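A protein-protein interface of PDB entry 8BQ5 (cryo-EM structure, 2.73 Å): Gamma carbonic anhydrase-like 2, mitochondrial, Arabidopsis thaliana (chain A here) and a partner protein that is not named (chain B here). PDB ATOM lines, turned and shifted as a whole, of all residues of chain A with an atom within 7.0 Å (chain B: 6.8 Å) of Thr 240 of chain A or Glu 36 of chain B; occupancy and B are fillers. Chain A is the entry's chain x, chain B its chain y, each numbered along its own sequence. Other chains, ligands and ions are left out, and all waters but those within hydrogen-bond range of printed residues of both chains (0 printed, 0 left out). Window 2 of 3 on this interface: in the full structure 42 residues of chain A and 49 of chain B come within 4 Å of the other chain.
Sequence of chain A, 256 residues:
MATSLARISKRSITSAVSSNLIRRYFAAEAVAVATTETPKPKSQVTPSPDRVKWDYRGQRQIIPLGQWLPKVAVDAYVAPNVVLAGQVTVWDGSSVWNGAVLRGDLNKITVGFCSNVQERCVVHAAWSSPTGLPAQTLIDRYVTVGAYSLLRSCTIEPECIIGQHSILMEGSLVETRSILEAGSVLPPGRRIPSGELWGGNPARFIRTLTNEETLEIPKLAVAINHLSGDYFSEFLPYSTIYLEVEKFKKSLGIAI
ND1 of His 38 of chain B sits at hydrogen-bond distance from OE1 of Glu 244 of chain A, at 3.5 Å. The side-chain hydroxyl of Ser 239 of chain A sits at hydrogen-bond distance from the side-chain carboxylate of Glu 37 of chain B (2.6 Å).
The backbone carbonyl oxygen (O) of Glu 36 of chain B sits close to a ring nitrogen (NE2) of His 38 of chain B, at 3.3 Å. NH2 of Arg 34 of chain B lies within salt-bridge range of OE1 of Glu 37 of chain B (2.8 Å).
Thr 240 of chain A touches Glu 36 of chain B. Ile 241 of chain A touches Glu 37 of chain B (CD1 to C, 3.3 Å). Ile 241 of chain A touches His 38 of chain B.
Of the printed residues of chain B, Ser 239 of chain A touches Glu 37. Of the printed residues of chain B, Ile 241 of chain A touches Glu 37 and His 38. Printed residues of chain B within 4 Å of Glu 244 of chain A: His 38. His 33 of chain B touches none of the printed residues of chain A. Of chain A, only Thr 240 comes within 4 Å of Glu 36 of chain B. The nearest printed residue of chain B that does not touch Ile 241 of chain A is Glu 36 of chain B (6.1 Å).
Of the 8 printed residues of chain A, 4 touch a printed residue of chain B. Hydrophobic or aromatic side chains of chain A within 4 Å of the printed part of chain B: Ile 241. Printed residues of chain B that touch a printed residue of chain A: Glu 36, Glu 37 and His 38. Among the printed residues, 5 pairs touch across the chains. Among the printed residues, no Asp or Glu carboxylate lies within 4 Å of a Lys or Arg side-chain nitrogen of the other chain.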
ATOM      1  N   TYR A 238      13.528 -10.497 -23.303  1.00  0.00           N
ATOM      2  CA  TYR A 238      13.106 -11.829 -22.899  1.00  0.00           C
ATOM      3  C   TYR A 238      11.634 -11.812 -22.516  1.00  0.00           C
ATOM      4  O   TYR A 238      11.128 -10.825 -21.973  1.00  0.00           O
ATOM      5  CB  TYR A 238      13.919 -12.339 -21.707  1.00  0.00           C
ATOM      6  CG  TYR A 238      15.308 -12.836 -22.027  1.00  0.00           C
ATOM      7  CD1 TYR A 238      16.374 -11.953 -22.121  1.00  0.00           C
ATOM      8  CD2 TYR A 238      15.564 -14.191 -22.189  1.00  0.00           C
ATOM      9  CE1 TYR A 238      17.648 -12.400 -22.391  1.00  0.00           C
ATOM     10  CE2 TYR A 238      16.838 -14.649 -22.459  1.00  0.00           C
ATOM     11  CZ  TYR A 238      17.876 -13.748 -22.559  1.00  0.00           C
ATOM     12  OH  TYR A 238      19.148 -14.190 -22.827  1.00  0.00           O
ATOM     13  N   SER A 239      10.954 -12.914 -22.797  1.00  0.00           N
ATOM     14  CA  SER A 239       9.599 -13.119 -22.316  1.00  0.00           C
ATOM     15  C   SER A 239       9.630 -13.718 -20.911  1.00  0.00           C
ATOM     16  O   SER A 239      10.675 -14.126 -20.404  1.00  0.00           O
ATOM     17  CB  SER A 239       8.826 -14.029 -23.272  1.00  0.00           C
ATOM     18  OG  SER A 239       7.439 -13.992 -22.993  1.00  0.00           O
ATOM     19  N   THR A 240       8.461 -13.760 -20.272  1.00  0.00           N
ATOM     20  CA  THR A 240       8.311 -14.394 -18.970  1.00  0.00           C
ATOM     21  C   THR A 240       7.612 -15.747 -19.059  1.00  0.00           C
ATOM     22  O   THR A 240       7.166 -16.275 -18.035  1.00  0.00           O
ATOM     23  CB  THR A 240       7.559 -13.472 -18.006  1.00  0.00           C
ATOM     24  OG1 THR A 240       6.458 -12.857 -18.685  1.00  0.00           O
ATOM     25  CG2 THR A 240       8.481 -12.392 -17.472  1.00  0.00           C
ATOM     26  N   ILE A 241       7.512 -16.319 -20.263  1.00  0.00           N
ATOM     27  CA  ILE A 241       6.812 -17.590 -20.442  1.00  0.00           C
ATOM     28  C   ILE A 241       7.549 -18.721 -19.741  1.00  0.00           C
ATOM     29  O   ILE A 241       6.931 -19.692 -19.283  1.00  0.00           O
ATOM     30  CB  ILE A 241       6.623 -17.895 -21.940  1.00  0.00           C
ATOM     31  CG1 ILE A 241       5.937 -16.730 -22.633  1.00  0.00           C
ATOM     32  CG2 ILE A 241       5.773 -19.139 -22.131  1.00  0.00           C
ATOM     33  CD1 ILE A 241       4.659 -16.366 -21.986  1.00  0.00           C
ATOM     34  N   TYR A 242       8.880 -18.631 -19.663  1.00  0.00           N
ATOM     35  CA  TYR A 242       9.646 -19.719 -19.066  1.00  0.00           C
ATOM     36  C   TYR A 242       9.249 -19.950 -17.615  1.00  0.00           C
ATOM     37  O   TYR A 242       9.313 -21.082 -17.130  1.00  0.00           O
ATOM     38  CB  TYR A 242      11.147 -19.450 -19.195  1.00  0.00           C
ATOM     39  CG  TYR A 242      11.684 -18.318 -18.347  1.00  0.00           C
ATOM     40  CD1 TYR A 242      11.695 -17.015 -18.821  1.00  0.00           C
ATOM     41  CD2 TYR A 242      12.210 -18.557 -17.083  1.00  0.00           C
ATOM     42  CE1 TYR A 242      12.192 -15.982 -18.057  1.00  0.00           C
ATOM     43  CE2 TYR A 242      12.712 -17.528 -16.311  1.00  0.00           C
ATOM     44  CZ  TYR A 242      12.700 -16.242 -16.804  1.00  0.00           C
ATOM     45  OH  TYR A 242      13.195 -15.207 -16.045  1.00  0.00           O
ATOM     46  N   LEU A 243       8.798 -18.905 -16.918  1.00  0.00           N
ATOM     47  CA  LEU A 243       8.302 -19.087 -15.558  1.00  0.00           C
ATOM     48  C   LEU A 243       6.998 -19.880 -15.547  1.00  0.00           C
ATOM     49  O   LEU A 243       6.780 -20.726 -14.668  1.00  0.00           O
ATOM     50  CB  LEU A 243       8.114 -17.728 -14.889  1.00  0.00           C
ATOM     51  CG  LEU A 243       9.402 -16.976 -14.559  1.00  0.00           C
ATOM     52  CD1 LEU A 243       9.083 -15.656 -13.888  1.00  0.00           C
ATOM     53  CD2 LEU A 243      10.323 -17.814 -13.690  1.00  0.00           C
ATOM     54  N   GLU A 244       6.116 -19.612 -16.514  1.00  0.00           N
ATOM     55  CA  GLU A 244       4.887 -20.389 -16.635  1.00  0.00           C
ATOM     56  C   GLU A 244       5.193 -21.849 -16.937  1.00  0.00           C
ATOM     57  O   GLU A 244       4.553 -22.753 -16.387  1.00  0.00           O
ATOM     58  CB  GLU A 244       3.993 -19.795 -17.722  1.00  0.00           C
ATOM     59  CG  GLU A 244       3.848 -18.292 -17.644  1.00  0.00           C
ATOM     60  CD  GLU A 244       2.580 -17.873 -16.938  1.00  0.00           C
ATOM     61  OE1 GLU A 244       1.556 -17.681 -17.626  1.00  0.00           O
ATOM     62  OE2 GLU A 244       2.607 -17.735 -15.698  1.00  0.00           O
ATOM     63  N   VAL A 245       6.172 -22.095 -17.810  1.00  0.00           N
ATOM     64  CA  VAL A 245       6.607 -23.463 -18.078  1.00  0.00           C
ATOM     65  C   VAL A 245       7.146 -24.105 -16.806  1.00  0.00           C
ATOM     66  O   VAL A 245       6.869 -25.277 -16.517  1.00  0.00           O
ATOM     67  CB  VAL A 245       7.654 -23.480 -19.207  1.00  0.00           C
ATOM     68  CG1 VAL A 245       8.059 -24.908 -19.532  1.00  0.00           C
ATOM     69  CG2 VAL A 245       7.123 -22.775 -20.441  1.00  0.00           C
ATOM     70  N   ASP B  23      10.177  -7.063 -10.836  1.00  0.00           N
ATOM     71  CA  ASP B  23       9.341  -7.152 -12.028  1.00  0.00           C
ATOM     72  C   ASP B  23       7.899  -6.782 -11.709  1.00  0.00           C
ATOM     73  O   ASP B  23       7.255  -6.043 -12.463  1.00  0.00           O
ATOM     74  CB  ASP B  23       9.427  -8.563 -12.609  1.00  0.00           C
ATOM     75  CG  ASP B  23       8.902  -8.650 -14.029  1.00  0.00           C
ATOM     76  OD1 ASP B  23       8.962  -7.641 -14.757  1.00  0.00           O
ATOM     77  OD2 ASP B  23       8.437  -9.741 -14.421  1.00  0.00           O
ATOM     78  N   SER B  27       5.704  -3.651 -13.102  1.00  0.00           N
ATOM     79  CA  SER B  27       4.391  -3.860 -13.708  1.00  0.00           C
ATOM     80  C   SER B  27       3.346  -2.951 -13.075  1.00  0.00           C
ATOM     81  O   SER B  27       2.489  -2.395 -13.771  1.00  0.00           O
ATOM     82  CB  SER B  27       3.971  -5.323 -13.570  1.00  0.00           C
ATOM     83  OG  SER B  27       4.865  -6.183 -14.250  1.00  0.00           O
ATOM     84  N   HIS B  33      -1.363  -1.955 -17.347  1.00  0.00           N
ATOM     85  CA  HIS B  33      -1.887  -1.804 -18.731  1.00  0.00           C
ATOM     86  C   HIS B  33      -1.352  -2.925 -19.622  1.00  0.00           C
ATOM     87  O   HIS B  33      -2.142  -3.451 -20.424  1.00  0.00           O
ATOM     88  CB  HIS B  33      -1.519  -0.433 -19.304  1.00  0.00           C
ATOM     89  CG  HIS B  33      -2.447   0.673 -18.934  1.00  0.00           C
ATOM     90  ND1 HIS B  33      -3.497   0.503 -18.056  1.00  0.00           N
ATOM     91  CD2 HIS B  33      -2.482   1.965 -19.323  1.00  0.00           C
ATOM     92  CE1 HIS B  33      -4.140   1.643 -17.920  1.00  0.00           C
ATOM     93  NE2 HIS B  33      -3.540   2.555 -18.691  1.00  0.00           N
ATOM     94  N   ARG B  34      -0.073  -3.282 -19.465  1.00  0.00           N
ATOM     95  CA  ARG B  34       0.539  -4.310 -20.343  1.00  0.00           C
ATOM     96  C   ARG B  34      -0.130  -5.659 -20.120  1.00  0.00           C
ATOM     97  O   ARG B  34      -0.193  -6.107 -18.969  1.00  0.00           O
ATOM     98  CB  ARG B  34       2.050  -4.443 -20.148  1.00  0.00           C
ATOM     99  CG  ARG B  34       2.723  -5.068 -21.361  1.00  0.00           C
ATOM    100  CD  ARG B  34       4.188  -5.411 -21.219  1.00  0.00           C
ATOM    101  NE  ARG B  34       4.676  -5.968 -22.472  1.00  0.00           N
ATOM    102  CZ  ARG B  34       4.726  -7.264 -22.757  1.00  0.00           C
ATOM    103  NH1 ARG B  34       4.334  -8.159 -21.868  1.00  0.00           N
ATOM    104  NH2 ARG B  34       5.180  -7.660 -23.931  1.00  0.00           N
ATOM    105  N   ILE B  35      -0.631  -6.259 -21.198  1.00  0.00           N
ATOM    106  CA  ILE B  35      -1.215  -7.628 -21.101  1.00  0.00           C
ATOM    107  C   ILE B  35      -0.041  -8.606 -21.057  1.00  0.00           C
ATOM    108  O   ILE B  35       0.898  -8.449 -21.833  1.00  0.00           O
ATOM    109  CB  ILE B  35      -2.210  -7.902 -22.245  1.00  0.00           C
ATOM    110  CG1 ILE B  35      -3.463  -7.033 -22.093  1.00  0.00           C
ATOM    111  CG2 ILE B  35      -2.565  -9.377 -22.332  1.00  0.00           C
ATOM    112  CD1 ILE B  35      -4.070  -6.580 -23.393  1.00  0.00           C
ATOM    113  N   GLU B  36      -0.064  -9.542 -20.125  1.00  0.00           N
ATOM    114  CA  GLU B  36       1.044 -10.470 -19.959  1.00  0.00           C
ATOM    115  C   GLU B  36       0.999 -11.563 -21.016  1.00  0.00           C
ATOM    116  O   GLU B  36      -0.071 -12.062 -21.371  1.00  0.00           O
ATOM    117  CB  GLU B  36       1.011 -11.094 -18.565  1.00  0.00           C
ATOM    118  CG  GLU B  36       1.297 -10.112 -17.446  1.00  0.00           C
ATOM    119  CD  GLU B  36       2.610 -10.391 -16.746  1.00  0.00           C
ATOM    120  OE1 GLU B  36       3.659 -10.386 -17.424  1.00  0.00           O
ATOM    121  OE2 GLU B  36       2.596 -10.608 -15.515  1.00  0.00           O
ATOM    122  N   GLU B  37       2.171 -11.921 -21.529  1.00  0.00           N
ATOM    123  CA  GLU B  37       2.286 -13.095 -22.380  1.00  0.00           C
ATOM    124  C   GLU B  37       2.078 -14.359 -21.549  1.00  0.00           C
ATOM    125  O   GLU B  37       2.482 -14.437 -20.386  1.00  0.00           O
ATOM    126  CB  GLU B  37       3.650 -13.119 -23.070  1.00  0.00           C
ATOM    127  CG  GLU B  37       3.888 -11.952 -24.016  1.00  0.00           C
ATOM    128  CD  GLU B  37       5.343 -11.534 -24.085  1.00  0.00           C
ATOM    129  OE1 GLU B  37       5.651 -10.380 -23.720  1.00  0.00           O
ATOM    130  OE2 GLU B  37       6.181 -12.357 -24.507  1.00  0.00           O
ATOM    131  N   HIS B  38       1.442 -15.358 -22.158  1.00  0.00           N
ATOM    132  CA  HIS B  38       1.073 -16.579 -21.453  1.00  0.00           C
ATOM    133  C   HIS B  38       1.547 -17.795 -22.236  1.00  0.00           C
ATOM    134  O   HIS B  38       2.028 -17.689 -23.367  1.00  0.00           O
ATOM    135  CB  HIS B  38      -0.441 -16.675 -21.228  1.00  0.00           C
ATOM    136  CG  HIS B  38      -0.989 -15.630 -20.309  1.00  0.00           C
ATOM    137  ND1 HIS B  38      -1.011 -15.779 -18.939  1.00  0.00           N
ATOM    138  CD2 HIS B  38      -1.562 -14.430 -20.565  1.00  0.00           C
ATOM    139  CE1 HIS B  38      -1.559 -14.711 -18.390  1.00  0.00           C
ATOM    140  NE2 HIS B  38      -1.901 -13.875 -19.355  1.00  0.00           N
